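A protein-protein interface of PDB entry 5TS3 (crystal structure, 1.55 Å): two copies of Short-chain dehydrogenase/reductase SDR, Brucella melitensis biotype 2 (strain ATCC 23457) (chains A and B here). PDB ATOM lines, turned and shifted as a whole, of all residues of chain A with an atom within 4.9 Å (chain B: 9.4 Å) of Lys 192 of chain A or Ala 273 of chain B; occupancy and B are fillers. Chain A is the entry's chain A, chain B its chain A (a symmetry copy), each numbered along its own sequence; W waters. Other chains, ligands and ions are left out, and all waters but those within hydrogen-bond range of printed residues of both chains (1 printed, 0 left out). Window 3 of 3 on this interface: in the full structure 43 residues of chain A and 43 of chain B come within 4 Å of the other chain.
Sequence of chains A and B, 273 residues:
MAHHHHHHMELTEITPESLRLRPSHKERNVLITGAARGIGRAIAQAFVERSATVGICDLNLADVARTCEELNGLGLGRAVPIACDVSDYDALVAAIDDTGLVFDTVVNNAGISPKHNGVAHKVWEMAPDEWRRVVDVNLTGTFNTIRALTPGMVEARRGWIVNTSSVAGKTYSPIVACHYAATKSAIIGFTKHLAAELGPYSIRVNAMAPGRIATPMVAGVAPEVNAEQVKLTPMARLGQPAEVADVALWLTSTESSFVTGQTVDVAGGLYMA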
ATOM      1  N   ILE A 188      18.111  10.312  -3.831  1.00  0.00           N
ATOM      2  CA  ILE A 188      18.377   8.947  -3.380  1.00  0.00           C
ATOM      3  C   ILE A 188      19.273   8.953  -2.141  1.00  0.00           C
ATOM      4  O   ILE A 188      18.936   8.358  -1.108  1.00  0.00           O
ATOM      5  CB  ILE A 188      18.983   8.128  -4.527  1.00  0.00           C
ATOM      6  CG1 ILE A 188      17.978   8.118  -5.685  1.00  0.00           C
ATOM      7  CG2 ILE A 188      19.280   6.707  -4.082  1.00  0.00           C
ATOM      8  CD1 ILE A 188      18.471   7.410  -6.891  1.00  0.00           C
ATOM      9  N   GLY A 189      20.427   9.619  -2.221  1.00  0.00           N
ATOM     10  CA  GLY A 189      21.315   9.658  -1.068  1.00  0.00           C
ATOM     11  C   GLY A 189      20.808  10.561   0.037  1.00  0.00           C
ATOM     12  O   GLY A 189      21.065  10.308   1.218  1.00  0.00           O
ATOM     13  N   PHE A 190      20.102  11.630  -0.330  1.00  0.00           N
ATOM     14  CA  PHE A 190      19.422  12.470   0.657  1.00  0.00           C
ATOM     15  C   PHE A 190      18.461  11.634   1.496  1.00  0.00           C
ATOM     16  O   PHE A 190      18.422  11.754   2.728  1.00  0.00           O
ATOM     17  CB  PHE A 190      18.674  13.584  -0.092  1.00  0.00           C
ATOM     18  CG  PHE A 190      18.035  14.659   0.773  1.00  0.00           C
ATOM     19  CD1 PHE A 190      18.575  15.069   1.994  1.00  0.00           C
ATOM     20  CD2 PHE A 190      16.899  15.302   0.303  1.00  0.00           C
ATOM     21  CE1 PHE A 190      17.964  16.086   2.730  1.00  0.00           C
ATOM     22  CE2 PHE A 190      16.283  16.312   1.027  1.00  0.00           C
ATOM     23  CZ  PHE A 190      16.812  16.711   2.241  1.00  0.00           C
ATOM     24  N   THR A 191      17.684  10.765   0.833  1.00  0.00           N
ATOM     25  CA  THR A 191      16.717   9.910   1.525  1.00  0.00           C
ATOM     26  C   THR A 191      17.408   8.933   2.481  1.00  0.00           C
ATOM     27  O   THR A 191      16.941   8.728   3.612  1.00  0.00           O
ATOM     28  CB  THR A 191      15.850   9.194   0.475  1.00  0.00           C
ATOM     29  OG1 THR A 191      15.042  10.183  -0.206  1.00  0.00           O
ATOM     30  CG2 THR A 191      14.951   8.114   1.083  1.00  0.00           C
ATOM     31  N   LYS A 192      18.527   8.333   2.067  1.00  0.00           N
ATOM     32  CA  LYS A 192      19.267   7.470   2.992  1.00  0.00           C
ATOM     33  C   LYS A 192      19.745   8.252   4.206  1.00  0.00           C
ATOM     34  O   LYS A 192      19.593   7.814   5.357  1.00  0.00           O
ATOM     35  CB  LYS A 192      20.470   6.838   2.291  1.00  0.00           C
ATOM     36  CG  LYS A 192      20.109   5.740   1.301  1.00  0.00           C
ATOM     37  CD  LYS A 192      21.371   5.150   0.691  1.00  0.00           C
ATOM     38  CE  LYS A 192      21.044   3.931  -0.152  1.00  0.00           C
ATOM     39  NZ  LYS A 192      20.288   4.329  -1.387  1.00  0.00           N
ATOM     40  N   HIS A 193      20.351   9.414   3.964  1.00  0.00           N
ATOM     41  CA  HIS A 193      20.888  10.213   5.062  1.00  0.00           C
ATOM     42  C   HIS A 193      19.786  10.623   6.031  1.00  0.00           C
ATOM     43  O   HIS A 193      19.930  10.494   7.254  1.00  0.00           O
ATOM     44  CB  HIS A 193      21.586  11.441   4.489  1.00  0.00           C
ATOM     45  CG  HIS A 193      22.299  12.245   5.521  1.00  0.00           C
ATOM     46  ND1 HIS A 193      23.659  12.154   5.733  1.00  0.00           N
ATOM     47  CD2 HIS A 193      21.825  13.111   6.448  1.00  0.00           C
ATOM     48  CE1 HIS A 193      23.994  12.949   6.736  1.00  0.00           C
ATOM     49  NE2 HIS A 193      22.899  13.543   7.183  1.00  0.00           N
ATOM     50  N   LEU A 194      18.668  11.107   5.493  1.00  0.00           N
ATOM     51  CA  LEU A 194      17.534  11.476   6.335  1.00  0.00           C
ATOM     52  C   LEU A 194      17.024  10.287   7.140  1.00  0.00           C
ATOM     53  O   LEU A 194      16.680  10.429   8.321  1.00  0.00           O
ATOM     54  CB  LEU A 194      16.414  12.041   5.464  1.00  0.00           C
ATOM     55  CG  LEU A 194      16.670  13.384   4.769  1.00  0.00           C
ATOM     56  CD1 LEU A 194      15.623  13.584   3.680  1.00  0.00           C
ATOM     57  CD2 LEU A 194      16.595  14.504   5.796  1.00  0.00           C
ATOM     58  N   ALA A 195      16.935   9.109   6.513  1.00  0.00           N
ATOM     59  CA  ALA A 195      16.465   7.932   7.238  1.00  0.00           C
ATOM     60  C   ALA A 195      17.344   7.656   8.448  1.00  0.00           C
ATOM     61  O   ALA A 195      16.852   7.260   9.512  1.00  0.00           O
ATOM     62  CB  ALA A 195      16.446   6.720   6.306  1.00  0.00           C
ATOM     63  N   ALA A 196      18.650   7.882   8.314  1.00  0.00           N
ATOM     64  CA  ALA A 196      19.541   7.610   9.431  1.00  0.00           C
ATOM     65  C   ALA A 196      19.390   8.660  10.523  1.00  0.00           C
ATOM     66  O   ALA A 196      19.438   8.327  11.712  1.00  0.00           O
ATOM     67  CB  ALA A 196      20.980   7.545   8.940  1.00  0.00           C
ATOM     68  N   GLY A 261      14.852   4.466   4.214  1.00  0.00           N
ATOM     69  CA  GLY A 261      16.002   4.812   3.401  1.00  0.00           C
ATOM     70  C   GLY A 261      15.953   4.297   1.979  1.00  0.00           C
ATOM     71  O   GLY A 261      16.929   4.485   1.235  1.00  0.00           O
ATOM     72  N   SER B 166      19.866  -9.790   1.083  1.00  0.00           N
ATOM     73  CA  SER B 166      20.282  -9.365   2.416  1.00  0.00           C
ATOM     74  C   SER B 166      21.044  -8.067   2.244  1.00  0.00           C
ATOM     75  O   SER B 166      21.640  -7.842   1.191  1.00  0.00           O
ATOM     76  CB  SER B 166      21.184 -10.400   3.108  1.00  0.00           C
ATOM     77  OG  SER B 166      21.800  -9.831   4.265  1.00  0.00           O
ATOM     78  N   VAL B 167      21.030  -7.219   3.278  1.00  0.00           N
ATOM     79  CA  VAL B 167      21.896  -6.041   3.204  1.00  0.00           C
ATOM     80  C   VAL B 167      23.352  -6.460   3.018  1.00  0.00           C
ATOM     81  O   VAL B 167      24.148  -5.717   2.424  1.00  0.00           O
ATOM     82  CB  VAL B 167      21.716  -5.124   4.434  1.00  0.00           C
ATOM     83  CG1 VAL B 167      20.292  -4.539   4.467  1.00  0.00           C
ATOM     84  CG2 VAL B 167      22.043  -5.851   5.738  1.00  0.00           C
ATOM     85  N   ALA B 168      23.720  -7.661   3.485  1.00  0.00           N
ATOM     86  CA  ALA B 168      25.085  -8.154   3.324  1.00  0.00           C
ATOM     87  C   ALA B 168      25.431  -8.492   1.881  1.00  0.00           C
ATOM     88  O   ALA B 168      26.612  -8.719   1.576  1.00  0.00           O
ATOM     89  CB  ALA B 168      25.301  -9.387   4.203  1.00  0.00           C
ATOM     90  N   GLY B 169      24.445  -8.547   0.992  1.00  0.00           N
ATOM     91  CA  GLY B 169      24.750  -8.691  -0.419  1.00  0.00           C
ATOM     92  C   GLY B 169      25.137  -7.402  -1.103  1.00  0.00           C
ATOM     93  O   GLY B 169      25.619  -7.438  -2.239  1.00  0.00           O
ATOM     94  N   LYS B 170      24.941  -6.258  -0.431  1.00  0.00           N
ATOM     95  CA  LYS B 170      25.251  -4.948  -0.990  1.00  0.00           C
ATOM     96  C   LYS B 170      26.357  -4.213  -0.263  1.00  0.00           C
ATOM     97  O   LYS B 170      26.927  -3.273  -0.825  1.00  0.00           O
ATOM     98  CB  LYS B 170      24.007  -4.047  -0.976  1.00  0.00           C
ATOM     99  CG  LYS B 170      23.022  -4.379  -2.044  1.00  0.00           C
ATOM    100  CD  LYS B 170      21.908  -3.379  -2.089  1.00  0.00           C
ATOM    101  CE  LYS B 170      20.924  -3.628  -0.987  1.00  0.00           C
ATOM    102  NZ  LYS B 170      20.035  -2.445  -0.871  1.00  0.00           N
ATOM    103  N   THR B 171      26.642  -4.577   0.976  1.00  0.00           N
ATOM    104  CA  THR B 171      27.759  -4.019   1.704  1.00  0.00           C
ATOM    105  C   THR B 171      28.183  -5.064   2.723  1.00  0.00           C
ATOM    106  O   THR B 171      27.521  -6.090   2.904  1.00  0.00           O
ATOM    107  CB  THR B 171      27.395  -2.676   2.351  1.00  0.00           C
ATOM    108  OG1 THR B 171      28.580  -2.048   2.860  1.00  0.00           O
ATOM    109  CG2 THR B 171      26.386  -2.879   3.471  1.00  0.00           C
ATOM    110  N   TYR B 172      29.303  -4.803   3.378  1.00  0.00           N
ATOM    111  CA  TYR B 172      29.920  -5.805   4.231  1.00  0.00           C
ATOM    112  C   TYR B 172      29.231  -5.898   5.578  1.00  0.00           C
ATOM    113  O   TYR B 172      29.071  -4.894   6.283  1.00  0.00           O
ATOM    114  CB  TYR B 172      31.384  -5.473   4.448  1.00  0.00           C
ATOM    115  CG  TYR B 172      32.098  -6.408   5.402  1.00  0.00           C
ATOM    116  CD1 TYR B 172      32.271  -7.754   5.092  1.00  0.00           C
ATOM    117  CD2 TYR B 172      32.642  -5.933   6.592  1.00  0.00           C
ATOM    118  CE1 TYR B 172      32.955  -8.602   5.949  1.00  0.00           C
ATOM    119  CE2 TYR B 172      33.329  -6.773   7.445  1.00  0.00           C
ATOM    120  CZ  TYR B 172      33.476  -8.105   7.126  1.00  0.00           C
ATOM    121  OH  TYR B 172      34.168  -8.939   7.988  1.00  0.00           O
ATOM    122  N   ILE B 188      20.189  -9.939  -6.357  1.00  0.00           N
ATOM    123  CA  ILE B 188      19.784  -8.595  -6.762  1.00  0.00           C
ATOM    124  C   ILE B 188      19.752  -8.476  -8.286  1.00  0.00           C
ATOM    125  O   ILE B 188      18.737  -8.075  -8.874  1.00  0.00           O
ATOM    126  CB  ILE B 188      20.712  -7.555  -6.121  1.00  0.00           C
ATOM    127  CG1 ILE B 188      20.611  -7.704  -4.599  1.00  0.00           C
ATOM    128  CG2 ILE B 188      20.319  -6.148  -6.534  1.00  0.00           C
ATOM    129  CD1 ILE B 188      21.515  -6.796  -3.853  1.00  0.00           C
ATOM    130  N   ALA B 209      15.669  -7.385   1.038  1.00  0.00           N
ATOM    131  CA  ALA B 209      17.000  -7.479   1.643  1.00  0.00           C
ATOM    132  C   ALA B 209      16.885  -7.141   3.123  1.00  0.00           C
ATOM    133  O   ALA B 209      17.108  -5.992   3.527  1.00  0.00           O
ATOM    134  CB  ALA B 209      18.002  -6.563   0.942  1.00  0.00           C
ATOM    135  N   PRO B 234      19.566   2.799  12.709  1.00  0.00           N
ATOM    136  CA  PRO B 234      18.884   4.058  13.060  1.00  0.00           C
ATOM    137  C   PRO B 234      17.597   3.862  13.844  1.00  0.00           C
ATOM    138  O   PRO B 234      17.383   4.570  14.834  1.00  0.00           O
ATOM    139  CB  PRO B 234      18.632   4.697  11.686  1.00  0.00           C
ATOM    140  CG  PRO B 234      19.802   4.224  10.843  1.00  0.00           C
ATOM    141  CD  PRO B 234      20.009   2.780  11.305  1.00  0.00           C
ATOM    142  N   THR B 263      14.888  -4.439  -5.331  1.00  0.00           N
ATOM    143  CA  THR B 263      15.317  -5.036  -4.069  1.00  0.00           C
ATOM    144  C   THR B 263      15.058  -3.998  -2.985  1.00  0.00           C
ATOM    145  O   THR B 263      15.659  -2.916  -2.996  1.00  0.00           O
ATOM    146  CB  THR B 263      16.783  -5.467  -4.107  1.00  0.00           C
ATOM    147  OG1 THR B 263      16.955  -6.497  -5.088  1.00  0.00           O
ATOM    148  CG2 THR B 263      17.219  -6.030  -2.741  1.00  0.00           C
ATOM    149  N   VAL B 264      14.145  -4.314  -2.074  1.00  0.00           N
ATOM    150  CA  VAL B 264      13.735  -3.406  -1.007  1.00  0.00           C
ATOM    151  C   VAL B 264      14.377  -3.883   0.288  1.00  0.00           C
ATOM    152  O   VAL B 264      14.094  -5.001   0.740  1.00  0.00           O
ATOM    153  CB  VAL B 264      12.207  -3.380  -0.872  1.00  0.00           C
ATOM    154  CG1 VAL B 264      11.776  -2.372   0.183  1.00  0.00           C
ATOM    155  CG2 VAL B 264      11.539  -3.107  -2.227  1.00  0.00           C
ATOM    156  N   ASP B 265      15.227  -3.052   0.900  1.00  0.00           N
ATOM    157  CA  ASP B 265      15.784  -3.427   2.199  1.00  0.00           C
ATOM    158  C   ASP B 265      14.695  -3.391   3.260  1.00  0.00           C
ATOM    159  O   ASP B 265      13.845  -2.493   3.273  1.00  0.00           O
ATOM    160  CB  ASP B 265      16.909  -2.485   2.641  1.00  0.00           C
ATOM    161  CG  ASP B 265      18.150  -2.543   1.761  1.00  0.00           C
ATOM    162  OD1 ASP B 265      18.150  -3.202   0.704  1.00  0.00           O
ATOM    163  OD2 ASP B 265      19.148  -1.872   2.138  1.00  0.00           O
ATOM    164  N   ALA B 267      15.239  -3.169   6.985  1.00  0.00           N
ATOM    165  CA  ALA B 267      16.435  -3.127   7.822  1.00  0.00           C
ATOM    166  C   ALA B 267      16.491  -1.951   8.782  1.00  0.00           C
ATOM    167  O   ALA B 267      17.493  -1.820   9.490  1.00  0.00           O
ATOM    168  CB  ALA B 267      17.688  -3.112   6.916  1.00  0.00           C
ATOM    169  N   GLY B 268      15.468  -1.097   8.831  1.00  0.00           N
ATOM    170  CA  GLY B 268      15.456  -0.017   9.800  1.00  0.00           C
ATOM    171  C   GLY B 268      16.602   0.964   9.668  1.00  0.00           C
ATOM    172  O   GLY B 268      16.936   1.651  10.641  1.00  0.00           O
ATOM    173  N   GLY B 269      17.223   1.040   8.490  1.00  0.00           N
ATOM    174  CA  GLY B 269      18.346   1.930   8.252  1.00  0.00           C
ATOM    175  C   GLY B 269      19.719   1.316   8.433  1.00  0.00           C
ATOM    176  O   GLY B 269      20.727   2.010   8.222  1.00  0.00           O
ATOM    177  N   LEU B 270      19.800   0.048   8.837  1.00  0.00           N
ATOM    178  CA  LEU B 270      21.090  -0.603   9.025  1.00  0.00           C
ATOM    179  C   LEU B 270      21.744  -0.900   7.682  1.00  0.00           C
ATOM    180  O   LEU B 270      21.117  -1.499   6.809  1.00  0.00           O
ATOM    181  CB  LEU B 270      20.893  -1.903   9.800  1.00  0.00           C
ATOM    182  CG  LEU B 270      22.146  -2.758   9.937  1.00  0.00           C
ATOM    183  CD1 LEU B 270      23.145  -2.070  10.836  1.00  0.00           C
ATOM    184  CD2 LEU B 270      21.760  -4.119  10.483  1.00  0.00           C
ATOM    185  N   TYR B 271      23.006  -0.491   7.520  1.00  0.00           N
ATOM    186  CA  TYR B 271      23.811  -0.883   6.354  1.00  0.00           C
ATOM    187  C   TYR B 271      23.128  -0.494   5.043  1.00  0.00           C
ATOM    188  O   TYR B 271      22.959  -1.320   4.136  1.00  0.00           O
ATOM    189  CB  TYR B 271      24.103  -2.389   6.363  1.00  0.00           C
ATOM    190  CG  TYR B 271      25.039  -2.892   7.457  1.00  0.00           C
ATOM    191  CD1 TYR B 271      26.032  -2.084   7.991  1.00  0.00           C
ATOM    192  CD2 TYR B 271      24.924  -4.193   7.939  1.00  0.00           C
ATOM    193  CE1 TYR B 271      26.883  -2.565   8.986  1.00  0.00           C
ATOM    194  CE2 TYR B 271      25.762  -4.677   8.918  1.00  0.00           C
ATOM    195  CZ  TYR B 271      26.741  -3.865   9.435  1.00  0.00           C
ATOM    196  OH  TYR B 271      27.572  -4.364  10.418  1.00  0.00           O
ATOM    197  N   MET B 272      22.714   0.770   4.943  1.00  0.00           N
ATOM    198  CA  MET B 272      22.052   1.215   3.724  1.00  0.00           C
ATOM    199  C   MET B 272      23.046   1.298   2.575  1.00  0.00           C
ATOM    200  O   MET B 272      24.185   1.754   2.736  1.00  0.00           O
ATOM    201  CB  MET B 272      21.372   2.570   3.928  1.00  0.00           C
ATOM    202  CG  MET B 272      20.131   2.485   4.780  1.00  0.00           C
ATOM    203  SD  MET B 272      19.325   4.079   5.100  1.00  0.00           S
ATOM    204  CE  MET B 272      20.468   4.839   6.251  1.00  0.00           C
ATOM    205  N   ALA B 273      22.606   0.829   1.415  1.00  0.00           N
ATOM    206  CA  ALA B 273      23.417   0.859   0.206  1.00  0.00           C
ATOM    207  C   ALA B 273      22.501   0.712  -1.004  1.00  0.00           C
ATOM    208  O   ALA B 273      21.414   0.128  -0.918  1.00  0.00           O
ATOM    209  CB  ALA B 273      24.463  -0.240   0.229  1.00  0.00           C
ATOM    210  OXT ALA B 273      22.831   1.182  -2.094  1.00  0.00           O
HETATM  211  O   HOH W   1      19.093   1.555  -1.272  1.00  0.00           O
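O of Lys 192 of chain A lies close to SD of Met 272 of chain B (3.8 Å).
NZ of Lys 170 of chain B is in salt-bridge range of O of Ala 273 of chain B (2.9 Å).
Lys 192 of chain A touches Ala 273 of chain B.
Pro 234 of chain B touches Ala 195 of chain A.
Pro 234 of chain B touches Ala 196 of chain A (CG to CA, 3.7 Å).
Met 272 of chain B touches Ala 196 of chain A.
Met 272 of chain B touches Gly 261 of chain A.
No residue of chain B comes within 4 Å of Gly 189 of chain A.
Thr 191 of chain A touches none of the printed residues of chain B.
Of chain B, only Met 272 and Ala 273 come within 4 Å of Lys 192 of chain A.
Of chain B, only Pro 234 comes within 4 Å of Ala 195 of chain A.
Of the printed residues of chain B, Ala 196 of chain A touches Pro 234 and Met 272.
Of the printed residues of chain B, Gly 261 of chain A touches Met 272 (3.8 Å).
Printed residues of chain A within 4 Å of Pro 234 of chain B: Ala 195 (3.8 Å) and Ala 196 (3.7 Å).
Of the printed residues of chain A, Met 272 of chain B touches Lys 192 (3.2 Å), Ala 196 (3.8 Å) and Gly 261 (3.8 Å).
The nearest printed residue of chain B that does not touch Lys 192 of chain A is Lys 170 of chain B (6.5 Å).
The nearest printed residue of chain A that does not touch Ala 273 of chain B is Gly 261 of chain A (6.6 Å).
The nearest printed residue of chain B that does not touch Gly 261 of chain A is Gly 269 of chain B (5.9 Å).
Of the 10 printed residues of chain A, 4 touch a printed residue of chain B.
Printed residues of chain A that touch a printed residue of chain B: Lys 192, Ala 195, Ala 196 and Gly 261.
Hydrophobic or aromatic side chains of chain A that line the printed part of chain B: Ala 196.
Of the 20 printed residues of chain B, 3 touch a printed residue of chain A.
Along chain B the printed residues that touch a printed residue of chain A span positions 234 to 273.
Among the printed residues, no Asp or Glu carboxylate lies within 4 Å of a Lys or Arg side-chain nitrogen of the other chain.
Position printed for both chains: 188.
Of the 6 pairs that touch across the chains among the printed residues, none has its exchanged pair printed and touching as well.
Water W1 bridges the chain-end carboxylate (O) of Ala 273 of chain B (2.7 Å) and the side-chain amino group (NZ) of Lys 192 of chain A (3.0 Å).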
